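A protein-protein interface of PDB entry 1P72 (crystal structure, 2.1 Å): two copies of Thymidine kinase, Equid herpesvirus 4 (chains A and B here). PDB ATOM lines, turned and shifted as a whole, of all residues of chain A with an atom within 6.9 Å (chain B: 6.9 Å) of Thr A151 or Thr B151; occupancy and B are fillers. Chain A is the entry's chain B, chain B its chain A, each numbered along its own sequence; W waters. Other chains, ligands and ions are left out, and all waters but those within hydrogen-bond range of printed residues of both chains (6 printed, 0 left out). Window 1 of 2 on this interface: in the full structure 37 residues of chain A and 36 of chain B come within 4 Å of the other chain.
The side-chain carboxylate (OD2) of Asp B96 lies within salt-bridge range of the side-chain amino group (NZ) of Lys A279 (2.8 Å). The side-chain amino group of Lys B279 lies within salt-bridge range of the side-chain carboxylate of Asp A96, 2.9 Å away.
The backbone carbonyl oxygen (O) of Ala B150 lies within hydrogen-bond range of the side-chain amino group (NZ) of Lys B279 (3.1 Å). O of Ala A150 is in hydrogen-bond range of NZ of Lys A279. OG1 of Thr A151 lies within hydrogen-bond range of O of Met A148 (2.8 Å). The backbone carbonyl oxygen (O) of Leu B152 lies within hydrogen-bond range of the side-chain amino group (NZ) of Lys B279, at 2.7 Å. The backbone carbonyl oxygen of Leu A152 lies within hydrogen-bond range of the side-chain amino group of Lys A279, 2.7 Å away. The backbone carbonyl oxygen (O) of Met B148 lies within hydrogen-bond range of the side-chain hydroxyl (OG1) of Thr B151.
Thr A89 touches Met B146 (CG2 to O, 3.8 Å). OG1 of Thr A89 touches CA of Ala B147, 3.3 Å away. Thr A89 touches Ala B150. Leu A92 touches Ala B150 (CD1 to O, 3.95 Å). Thr B151 touches Leu A92 (CG2 to CD1, 3.7 Å). Thr B89 touches Met A146. Ala A147 touches Thr B89 (CB to OG1, 3.4 Å). Asp B96 touches Ala A150 (OD2 to O, 3.96 Å). Thr A151 touches Leu B92 (CG2 to CD1, 3.8 Å). CG2 of Thr A151 touches CG2 of Thr B151 (3.7 Å).
Thr A151 touches two residues of chain B. Of chain A, only Leu A92 (3.7 Å) and Thr A151 (3.7 Å) come within 4 Å of Thr B151. Of the printed residues of chain A, Lys B279 touches Asp A96 (2.9 Å). Printed residues of chain B within 4 Å of Ala A147: Thr B89 (3.4 Å). The nearest residue of chain A that does not touch Thr B151 is Thr A88 (5.3 Å).
Printed residues of chain B that touch a printed residue of chain A: Thr B89, Leu B92, Asp B96, Met B146, Ala B147, Ala B150, Thr B151 and Lys B279. Hydrophobic or aromatic side chains of chain B that line the printed part of chain A: Leu B92, Ala B147 and Ala B150. Printed residues of chain A that touch a printed residue of chain B: Thr A89, Leu A92, Asp A96, Met A146, Ala A147, Ala A150, Thr A151 and Lys A279. Hydrophobic or aromatic side chains of chain A within 4 Å of the printed part of chain B: Leu A92 and Ala A147. Among the printed residues, Asp or Glu carboxylates within 4 Å of a Lys or Arg side-chain nitrogen of the other chain: Asp A96 with Lys B279 (2.9 Å) and Lys A279 with Asp B96 (2.8 Å).
Thr A89 touches Met B146, and with the chains exchanged Met A146 touches Thr B89. Leu A92 touches Thr B151, and with the chains exchanged Thr A151 touches Leu B92. Asp A96 touches Lys B279, and with the chains exchanged Lys A279 touches Asp B96. Thr B151 touches its own counterpart, Thr A151. Positions printed for both chains: 85, 88, 89, 92, 96, 123, 126, 127, 146, 147, 148, 149, 150, 151, 152, 153, 154 and 279.
Water W1 lies within hydrogen-bond range of O of Ala B147, OG1 of Thr A89 and OG1 of Thr A88. Water W3 lies within hydrogen-bond range of the side-chain hydroxyl (OG) of Ser A85 (2.6 Å) and the side-chain hydroxyl (OG) of Ser B85 (2.9 Å). Water W4 lies within hydrogen-bond range of OD1 of Asp A96 and NZ of Lys B279. Water W2 lies within hydrogen-bond range of the backbone carbonyl oxygen (O) of Ala A147 (2.7 Å), the side-chain hydroxyl (OG1) of Thr B89 (2.9 Å) and the side-chain hydroxyl (OG1) of Thr B88 (3.2 Å). Water W5 lies within hydrogen-bond range of O of Ala B150 (2.8 Å), NZ of Lys B279 (3.5 Å) and OD2 of Asp A96 (3.5 Å). Water W6 bridges OD1 of Asp B96 and NZ of Lys A279.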
ATOM      1  N   SER A  85       0.441   5.512 -32.671  1.00  0.00           N
ATOM      2  CA  SER A  85       1.220   6.111 -31.578  1.00  0.00           C
ATOM      3  C   SER A  85       1.208   7.633 -31.651  1.00  0.00           C
ATOM      4  O   SER A  85       1.077   8.304 -30.625  1.00  0.00           O
ATOM      5  CB  SER A  85       2.685   5.625 -31.562  1.00  0.00           C
ATOM      6  OG  SER A  85       2.754   4.228 -31.308  1.00  0.00           O
ATOM      7  N   THR A  88      -1.586   9.638 -30.092  1.00  0.00           N
ATOM      8  CA  THR A  88      -1.671   9.764 -28.634  1.00  0.00           C
ATOM      9  C   THR A  88      -0.898  10.958 -28.137  1.00  0.00           C
ATOM     10  O   THR A  88      -1.299  11.587 -27.162  1.00  0.00           O
ATOM     11  CB  THR A  88      -1.203   8.480 -27.878  1.00  0.00           C
ATOM     12  OG1 THR A  88       0.206   8.312 -28.049  1.00  0.00           O
ATOM     13  CG2 THR A  88      -1.780   7.235 -28.497  1.00  0.00           C
ATOM     14  N   THR A  89       0.202  11.294 -28.823  1.00  0.00           N
ATOM     15  CA  THR A  89       1.158  12.261 -28.283  1.00  0.00           C
ATOM     16  C   THR A  89       0.549  13.512 -27.654  1.00  0.00           C
ATOM     17  O   THR A  89       0.840  13.819 -26.493  1.00  0.00           O
ATOM     18  CB  THR A  89       2.237  12.629 -29.340  1.00  0.00           C
ATOM     19  OG1 THR A  89       2.768  11.425 -29.900  1.00  0.00           O
ATOM     20  CG2 THR A  89       3.450  13.282 -28.665  1.00  0.00           C
ATOM     21  N   LEU A  92      -1.306  12.850 -24.465  1.00  0.00           N
ATOM     22  CA  LEU A  92      -0.359  12.610 -23.359  1.00  0.00           C
ATOM     23  C   LEU A  92       0.185  13.934 -22.807  1.00  0.00           C
ATOM     24  O   LEU A  92       0.274  14.124 -21.578  1.00  0.00           O
ATOM     25  CB  LEU A  92       0.788  11.713 -23.830  1.00  0.00           C
ATOM     26  CG  LEU A  92       0.364  10.272 -24.132  1.00  0.00           C
ATOM     27  CD1 LEU A  92       1.526   9.357 -24.456  1.00  0.00           C
ATOM     28  CD2 LEU A  92      -0.474   9.679 -22.998  1.00  0.00           C
ATOM     29  N   ASP A  96      -0.639  15.289 -19.127  1.00  0.00           N
ATOM     30  CA  ASP A  96       0.477  15.684 -18.263  1.00  0.00           C
ATOM     31  C   ASP A  96       0.378  17.146 -17.775  1.00  0.00           C
ATOM     32  O   ASP A  96       0.750  17.453 -16.640  1.00  0.00           O
ATOM     33  CB  ASP A  96       1.821  15.489 -18.970  1.00  0.00           C
ATOM     34  CG  ASP A  96       2.330  14.057 -18.891  1.00  0.00           C
ATOM     35  OD1 ASP A  96       2.018  13.329 -17.907  1.00  0.00           O
ATOM     36  OD2 ASP A  96       3.059  13.566 -19.780  1.00  0.00           O
ATOM     37  N   PRO A 123      -7.366  10.351 -23.126  1.00  0.00           N
ATOM     38  CA  PRO A 123      -6.283   9.516 -23.679  1.00  0.00           C
ATOM     39  C   PRO A 123      -6.625   8.041 -23.949  1.00  0.00           C
ATOM     40  O   PRO A 123      -5.982   7.437 -24.779  1.00  0.00           O
ATOM     41  CB  PRO A 123      -5.162   9.653 -22.638  1.00  0.00           C
ATOM     42  CG  PRO A 123      -5.408  11.056 -22.082  1.00  0.00           C
ATOM     43  CD  PRO A 123      -6.905  11.159 -21.975  1.00  0.00           C
ATOM     44  N   SER A 126      -7.018   7.160 -27.902  1.00  0.00           N
ATOM     45  CA  SER A 126      -5.878   6.874 -28.798  1.00  0.00           C
ATOM     46  C   SER A 126      -4.925   5.786 -28.315  1.00  0.00           C
ATOM     47  O   SER A 126      -4.173   5.223 -29.134  1.00  0.00           O
ATOM     48  CB  SER A 126      -5.084   8.154 -29.065  1.00  0.00           C
ATOM     49  OG  SER A 126      -4.629   8.728 -27.840  1.00  0.00           O
ATOM     50  N   THR A 127      -4.902   5.515 -26.993  1.00  0.00           N
ATOM     51  CA  THR A 127      -3.999   4.495 -26.457  1.00  0.00           C
ATOM     52  C   THR A 127      -4.625   3.103 -26.385  1.00  0.00           C
ATOM     53  O   THR A 127      -3.889   2.109 -26.331  1.00  0.00           O
ATOM     54  CB  THR A 127      -3.421   4.840 -25.033  1.00  0.00           C
ATOM     55  OG1 THR A 127      -4.490   5.062 -24.095  1.00  0.00           O
ATOM     56  CG2 THR A 127      -2.585   6.149 -25.027  1.00  0.00           C
ATOM     57  N   MET A 146      -0.455  -3.948 -27.236  1.00  0.00           N
ATOM     58  CA  MET A 146       0.196  -3.838 -25.917  1.00  0.00           C
ATOM     59  C   MET A 146       0.995  -2.565 -25.801  1.00  0.00           C
ATOM     60  O   MET A 146       0.920  -1.872 -24.780  1.00  0.00           O
ATOM     61  CB  MET A 146       1.115  -5.025 -25.633  1.00  0.00           C
ATOM     62  CG  MET A 146       0.387  -6.239 -25.113  1.00  0.00           C
ATOM     63  SD  MET A 146      -0.557  -5.881 -23.606  1.00  0.00           S
ATOM     64  CE  MET A 146      -1.110  -7.503 -23.267  1.00  0.00           C
ATOM     65  N   ALA A 147       1.738  -2.246 -26.858  1.00  0.00           N
ATOM     66  CA  ALA A 147       2.601  -1.079 -26.859  1.00  0.00           C
ATOM     67  C   ALA A 147       1.812   0.194 -26.647  1.00  0.00           C
ATOM     68  O   ALA A 147       2.296   1.090 -25.954  1.00  0.00           O
ATOM     69  CB  ALA A 147       3.436  -0.983 -28.165  1.00  0.00           C
ATOM     70  N   MET A 148       0.629   0.298 -27.268  1.00  0.00           N
ATOM     71  CA  MET A 148      -0.236   1.474 -27.084  1.00  0.00           C
ATOM     72  C   MET A 148      -0.889   1.487 -25.711  1.00  0.00           C
ATOM     73  O   MET A 148      -0.963   2.533 -25.074  1.00  0.00           O
ATOM     74  CB  MET A 148      -1.383   1.542 -28.125  1.00  0.00           C
ATOM     75  CG  MET A 148      -1.093   0.945 -29.504  1.00  0.00           C
ATOM     76  SD  MET A 148      -0.906   2.219 -30.736  1.00  0.00           S
ATOM     77  CE  MET A 148       0.444   2.974 -29.940  1.00  0.00           C
ATOM     78  N   VAL A 149      -1.398   0.329 -25.295  1.00  0.00           N
ATOM     79  CA  VAL A 149      -2.160   0.220 -24.051  1.00  0.00           C
ATOM     80  C   VAL A 149      -1.276   0.586 -22.837  1.00  0.00           C
ATOM     81  O   VAL A 149      -1.737   1.279 -21.933  1.00  0.00           O
ATOM     82  CB  VAL A 149      -2.811  -1.193 -23.889  1.00  0.00           C
ATOM     83  CG1 VAL A 149      -3.369  -1.407 -22.469  1.00  0.00           C
ATOM     84  CG2 VAL A 149      -3.957  -1.396 -24.922  1.00  0.00           C
ATOM     85  N   ALA A 150      -0.014   0.122 -22.842  1.00  0.00           N
ATOM     86  CA  ALA A 150       0.933   0.424 -21.768  1.00  0.00           C
ATOM     87  C   ALA A 150       1.172   1.929 -21.553  1.00  0.00           C
ATOM     88  O   ALA A 150       1.528   2.319 -20.454  1.00  0.00           O
ATOM     89  CB  ALA A 150       2.284  -0.337 -21.962  1.00  0.00           C
ATOM     90  N   THR A 151       0.964   2.756 -22.589  1.00  0.00           N
ATOM     91  CA  THR A 151       1.170   4.217 -22.511  1.00  0.00           C
ATOM     92  C   THR A 151      -0.059   4.974 -22.019  1.00  0.00           C
ATOM     93  O   THR A 151      -0.024   6.193 -21.895  1.00  0.00           O
ATOM     94  CB  THR A 151       1.655   4.855 -23.874  1.00  0.00           C
ATOM     95  OG1 THR A 151       0.557   4.866 -24.809  1.00  0.00           O
ATOM     96  CG2 THR A 151       2.729   4.006 -24.574  1.00  0.00           C
ATOM     97  N   LEU A 152      -1.144   4.268 -21.707  1.00  0.00           N
ATOM     98  CA  LEU A 152      -2.295   4.919 -21.074  1.00  0.00           C
ATOM     99  C   LEU A 152      -1.825   5.525 -19.762  1.00  0.00           C
ATOM    100  O   LEU A 152      -1.176   4.839 -18.973  1.00  0.00           O
ATOM    101  CB  LEU A 152      -3.366   3.892 -20.757  1.00  0.00           C
ATOM    102  CG  LEU A 152      -4.892   4.103 -20.613  1.00  0.00           C
ATOM    103  CD1 LEU A 152      -5.487   3.387 -19.375  1.00  0.00           C
ATOM    104  CD2 LEU A 152      -5.473   5.475 -20.804  1.00  0.00           C
ATOM    105  N   PRO A 153      -2.135   6.799 -19.525  1.00  0.00           N
ATOM    106  CA  PRO A 153      -1.804   7.432 -18.242  1.00  0.00           C
ATOM    107  C   PRO A 153      -2.854   7.129 -17.179  1.00  0.00           C
ATOM    108  O   PRO A 153      -4.025   6.909 -17.524  1.00  0.00           O
ATOM    109  CB  PRO A 153      -1.792   8.926 -18.575  1.00  0.00           C
ATOM    110  CG  PRO A 153      -2.739   9.071 -19.757  1.00  0.00           C
ATOM    111  CD  PRO A 153      -2.756   7.744 -20.481  1.00  0.00           C
ATOM    112  N   ARG A 154      -2.447   7.114 -15.914  1.00  0.00           N
ATOM    113  CA  ARG A 154      -3.389   6.900 -14.815  1.00  0.00           C
ATOM    114  C   ARG A 154      -4.247   8.152 -14.656  1.00  0.00           C
ATOM    115  O   ARG A 154      -3.730   9.275 -14.637  1.00  0.00           O
ATOM    116  CB  ARG A 154      -2.624   6.630 -13.495  1.00  0.00           C
ATOM    117  CG  ARG A 154      -3.514   6.297 -12.266  1.00  0.00           C
ATOM    118  CD  ARG A 154      -2.699   6.212 -10.949  1.00  0.00           C
ATOM    119  NE  ARG A 154      -2.283   7.568 -10.569  1.00  0.00           N
ATOM    120  CZ  ARG A 154      -2.994   8.389  -9.792  1.00  0.00           C
ATOM    121  NH1 ARG A 154      -4.126   7.972  -9.239  1.00  0.00           N
ATOM    122  NH2 ARG A 154      -2.545   9.616  -9.538  1.00  0.00           N
ATOM    123  N   LYS A 279      -5.689   2.196 -14.000  1.00  0.00           N
ATOM    124  CA  LYS A 279      -5.732   3.486 -14.697  1.00  0.00           C
ATOM    125  C   LYS A 279      -7.153   3.937 -15.031  1.00  0.00           C
ATOM    126  O   LYS A 279      -7.377   5.122 -15.189  1.00  0.00           O
ATOM    127  CB  LYS A 279      -4.879   3.456 -15.958  1.00  0.00           C
ATOM    128  CG  LYS A 279      -3.389   3.241 -15.651  1.00  0.00           C
ATOM    129  CD  LYS A 279      -2.613   2.763 -16.905  1.00  0.00           C
ATOM    130  CE  LYS A 279      -1.113   2.800 -16.615  1.00  0.00           C
ATOM    131  NZ  LYS A 279      -0.399   2.470 -17.864  1.00  0.00           N
ATOM    132  N   SER B  85       9.356   2.079 -30.111  1.00  0.00           N
ATOM    133  CA  SER B  85       8.174   2.021 -29.266  1.00  0.00           C
ATOM    134  C   SER B  85       8.108   0.702 -28.535  1.00  0.00           C
ATOM    135  O   SER B  85       7.818   0.677 -27.337  1.00  0.00           O
ATOM    136  CB  SER B  85       6.891   2.193 -30.095  1.00  0.00           C
ATOM    137  OG  SER B  85       6.625   3.566 -30.305  1.00  0.00           O
ATOM    138  N   THR B  88      10.067   0.007 -25.372  1.00  0.00           N
ATOM    139  CA  THR B  88       9.642   0.641 -24.132  1.00  0.00           C
ATOM    140  C   THR B  88       8.616  -0.174 -23.372  1.00  0.00           C
ATOM    141  O   THR B  88       8.547  -0.065 -22.151  1.00  0.00           O
ATOM    142  CB  THR B  88       9.086   2.072 -24.337  1.00  0.00           C
ATOM    143  OG1 THR B  88       7.835   2.004 -25.027  1.00  0.00           O
ATOM    144  CG2 THR B  88       9.973   2.871 -25.241  1.00  0.00           C
ATOM    145  N   THR B  89       7.851  -0.994 -24.104  1.00  0.00           N
ATOM    146  CA  THR B  89       6.655  -1.662 -23.576  1.00  0.00           C
ATOM    147  C   THR B  89       6.863  -2.362 -22.243  1.00  0.00           C
ATOM    148  O   THR B  89       6.168  -2.031 -21.283  1.00  0.00           O
ATOM    149  CB  THR B  89       6.009  -2.627 -24.646  1.00  0.00           C
ATOM    150  OG1 THR B  89       5.776  -1.885 -25.846  1.00  0.00           O
ATOM    151  CG2 THR B  89       4.583  -3.038 -24.225  1.00  0.00           C
ATOM    152  N   LEU B  92       7.543  -0.082 -19.357  1.00  0.00           N
ATOM    153  CA  LEU B  92       6.333   0.597 -18.874  1.00  0.00           C
ATOM    154  C   LEU B  92       5.490  -0.311 -17.997  1.00  0.00           C
ATOM    155  O   LEU B  92       5.009   0.119 -16.943  1.00  0.00           O
ATOM    156  CB  LEU B  92       5.503   1.173 -20.022  1.00  0.00           C
ATOM    157  CG  LEU B  92       6.206   2.234 -20.885  1.00  0.00           C
ATOM    158  CD1 LEU B  92       5.271   2.745 -21.991  1.00  0.00           C
ATOM    159  CD2 LEU B  92       6.692   3.375 -20.022  1.00  0.00           C
ATOM    160  N   ASP B  96       4.923   0.257 -13.994  1.00  0.00           N
ATOM    161  CA  ASP B  96       3.535   0.314 -13.515  1.00  0.00           C
ATOM    162  C   ASP B  96       3.341  -0.688 -12.394  1.00  0.00           C
ATOM    163  O   ASP B  96       2.694  -0.384 -11.400  1.00  0.00           O
ATOM    164  CB  ASP B  96       2.512  -0.005 -14.625  1.00  0.00           C
ATOM    165  CG  ASP B  96       2.091   1.234 -15.448  1.00  0.00           C
ATOM    166  OD1 ASP B  96       2.034   2.353 -14.889  1.00  0.00           O
ATOM    167  OD2 ASP B  96       1.773   1.173 -16.669  1.00  0.00           O
ATOM    168  N   PRO B 123      12.929   3.340 -17.531  1.00  0.00           N
ATOM    169  CA  PRO B 123      12.167   3.696 -18.742  1.00  0.00           C
ATOM    170  C   PRO B 123      12.732   4.856 -19.577  1.00  0.00           C
ATOM    171  O   PRO B 123      12.429   4.918 -20.771  1.00  0.00           O
ATOM    172  CB  PRO B 123      10.791   4.038 -18.183  1.00  0.00           C
ATOM    173  CG  PRO B 123      10.652   3.099 -16.990  1.00  0.00           C
ATOM    174  CD  PRO B 123      12.028   3.168 -16.366  1.00  0.00           C
ATOM    175  N   SER B 126      14.573   3.853 -23.104  1.00  0.00           N
ATOM    176  CA  SER B 126      13.834   3.450 -24.297  1.00  0.00           C
ATOM    177  C   SER B 126      12.886   4.557 -24.735  1.00  0.00           C
ATOM    178  O   SER B 126      12.501   4.638 -25.894  1.00  0.00           O
ATOM    179  CB  SER B 126      13.116   2.096 -24.065  1.00  0.00           C
ATOM    180  OG  SER B 126      12.150   2.171 -23.005  1.00  0.00           O
ATOM    181  N   THR B 127      12.531   5.451 -23.824  1.00  0.00           N
ATOM    182  CA  THR B 127      11.601   6.501 -24.212  1.00  0.00           C
ATOM    183  C   THR B 127      12.291   7.781 -24.585  1.00  0.00           C
ATOM    184  O   THR B 127      11.689   8.632 -25.250  1.00  0.00           O
ATOM    185  CB  THR B 127      10.562   6.799 -23.114  1.00  0.00           C
ATOM    186  OG1 THR B 127      11.221   7.157 -21.888  1.00  0.00           O
ATOM    187  CG2 THR B 127       9.742   5.543 -22.812  1.00  0.00           C
ATOM    188  N   MET B 146       9.277  13.105 -30.072  1.00  0.00           N
ATOM    189  CA  MET B 146       8.255  13.603 -29.152  1.00  0.00           C
ATOM    190  C   MET B 146       7.288  12.519 -28.708  1.00  0.00           C
ATOM    191  O   MET B 146       6.950  12.440 -27.531  1.00  0.00           O
ATOM    192  CB  MET B 146       7.455  14.734 -29.766  1.00  0.00           C
ATOM    193  CG  MET B 146       8.169  16.050 -29.698  1.00  0.00           C
ATOM    194  SD  MET B 146       8.385  16.675 -27.992  1.00  0.00           S
ATOM    195  CE  MET B 146       7.016  15.993 -27.066  1.00  0.00           C
ATOM    196  N   ALA B 147       6.865  11.692 -29.662  1.00  0.00           N
ATOM    197  CA  ALA B 147       5.907  10.632 -29.404  1.00  0.00           C
ATOM    198  C   ALA B 147       6.455   9.723 -28.345  1.00  0.00           C
ATOM    199  O   ALA B 147       5.723   9.319 -27.439  1.00  0.00           O
ATOM    200  CB  ALA B 147       5.611   9.859 -30.653  1.00  0.00           C
ATOM    201  N   MET B 148       7.755   9.424 -28.442  1.00  0.00           N
ATOM    202  CA  MET B 148       8.412   8.562 -27.463  1.00  0.00           C
ATOM    203  C   MET B 148       8.613   9.253 -26.115  1.00  0.00           C
ATOM    204  O   MET B 148       8.279   8.696 -25.068  1.00  0.00           O
ATOM    205  CB  MET B 148       9.782   8.109 -28.000  1.00  0.00           C
ATOM    206  CG  MET B 148       9.745   7.395 -29.341  1.00  0.00           C
ATOM    207  SD  MET B 148       8.769   5.885 -29.263  1.00  0.00           S
ATOM    208  CE  MET B 148       9.613   4.991 -27.887  1.00  0.00           C
ATOM    209  N   VAL B 149       9.124  10.482 -26.151  1.00  0.00           N
ATOM    210  CA  VAL B 149       9.418  11.200 -24.918  1.00  0.00           C
ATOM    211  C   VAL B 149       8.136  11.357 -24.104  1.00  0.00           C
ATOM    212  O   VAL B 149       8.153  11.247 -22.863  1.00  0.00           O
ATOM    213  CB  VAL B 149      10.044  12.580 -25.206  1.00  0.00           C
ATOM    214  CG1 VAL B 149       9.991  13.470 -23.976  1.00  0.00           C
ATOM    215  CG2 VAL B 149      11.468  12.412 -25.700  1.00  0.00           C
ATOM    216  N   ALA B 150       7.028  11.616 -24.804  1.00  0.00           N
ATOM    217  CA  ALA B 150       5.752  11.803 -24.111  1.00  0.00           C
ATOM    218  C   ALA B 150       5.328  10.586 -23.248  1.00  0.00           C
ATOM    219  O   ALA B 150       4.551  10.726 -22.310  1.00  0.00           O
ATOM    220  CB  ALA B 150       4.656  12.179 -25.112  1.00  0.00           C
ATOM    221  N   THR B 151       5.807   9.393 -23.600  1.00  0.00           N
ATOM    222  CA  THR B 151       5.390   8.169 -22.907  1.00  0.00           C
ATOM    223  C   THR B 151       6.301   7.824 -21.707  1.00  0.00           C
ATOM    224  O   THR B 151       6.056   6.831 -21.035  1.00  0.00           O
ATOM    225  CB  THR B 151       5.309   6.931 -23.853  1.00  0.00           C
ATOM    226  OG1 THR B 151       6.640   6.560 -24.266  1.00  0.00           O
ATOM    227  CG2 THR B 151       4.517   7.237 -25.200  1.00  0.00           C
ATOM    228  N   LEU B 152       7.355   8.603 -21.467  1.00  0.00           N
ATOM    229  CA  LEU B 152       8.138   8.467 -20.222  1.00  0.00           C
ATOM    230  C   LEU B 152       7.191   8.524 -19.000  1.00  0.00           C
ATOM    231  O   LEU B 152       6.422   9.460 -18.897  1.00  0.00           O
ATOM    232  CB  LEU B 152       9.103   9.645 -20.124  1.00  0.00           C
ATOM    233  CG  LEU B 152      10.475   9.628 -19.422  1.00  0.00           C
ATOM    234  CD1 LEU B 152      10.687  10.879 -18.596  1.00  0.00           C
ATOM    235  CD2 LEU B 152      10.864   8.345 -18.667  1.00  0.00           C
ATOM    236  N   PRO B 153       7.223   7.546 -18.092  1.00  0.00           N
ATOM    237  CA  PRO B 153       6.403   7.637 -16.871  1.00  0.00           C
ATOM    238  C   PRO B 153       7.073   8.526 -15.819  1.00  0.00           C
ATOM    239  O   PRO B 153       8.301   8.563 -15.764  1.00  0.00           O
ATOM    240  CB  PRO B 153       6.348   6.188 -16.380  1.00  0.00           C
ATOM    241  CG  PRO B 153       7.631   5.555 -16.878  1.00  0.00           C
ATOM    242  CD  PRO B 153       7.981   6.280 -18.161  1.00  0.00           C
ATOM    243  N   ARG B 154       6.274   9.231 -15.023  1.00  0.00           N
ATOM    244  CA  ARG B 154       6.763   9.999 -13.895  1.00  0.00           C
ATOM    245  C   ARG B 154       7.404   9.064 -12.887  1.00  0.00           C
ATOM    246  O   ARG B 154       6.818   8.043 -12.497  1.00  0.00           O
ATOM    247  CB  ARG B 154       5.606  10.715 -13.195  1.00  0.00           C
ATOM    248  CG  ARG B 154       6.058  11.651 -12.064  1.00  0.00           C
ATOM    249  CD  ARG B 154       4.912  12.305 -11.306  1.00  0.00           C
ATOM    250  NE  ARG B 154       4.255  11.325 -10.455  1.00  0.00           N
ATOM    251  CZ  ARG B 154       4.585  11.066  -9.190  1.00  0.00           C
ATOM    252  NH1 ARG B 154       5.551  11.743  -8.579  1.00  0.00           N
ATOM    253  NH2 ARG B 154       3.916  10.132  -8.528  1.00  0.00           N
ATOM    254  N   LYS B 279       9.086  14.638 -14.749  1.00  0.00           N
ATOM    255  CA  LYS B 279       9.184  13.189 -14.710  1.00  0.00           C
ATOM    256  C   LYS B 279      10.552  12.726 -14.233  1.00  0.00           C
ATOM    257  O   LYS B 279      10.667  11.630 -13.665  1.00  0.00           O
ATOM    258  CB  LYS B 279       8.858  12.576 -16.072  1.00  0.00           C
ATOM    259  CG  LYS B 279       7.372  12.690 -16.438  1.00  0.00           C
ATOM    260  CD  LYS B 279       7.149  12.469 -17.930  1.00  0.00           C
ATOM    261  CE  LYS B 279       5.644  12.500 -18.234  1.00  0.00           C
ATOM    262  NZ  LYS B 279       5.355  11.867 -19.563  1.00  0.00           N
HETATM  263  O   HOH W   1       3.165   9.560 -27.843  1.00  0.00           O
HETATM  264  O   HOH W   2       4.866   0.721 -25.052  1.00  0.00           O
HETATM  265  O   HOH W   3       4.827   3.199 -32.536  1.00  0.00           O
HETATM  266  O   HOH W   4       2.692  10.744 -18.098  1.00  0.00           O
HETATM  267  O   HOH W   5       2.466  10.216 -20.488  1.00  0.00           O
HETATM  268  O   HOH W   6       1.813   4.610 -16.616  1.00  0.00           O
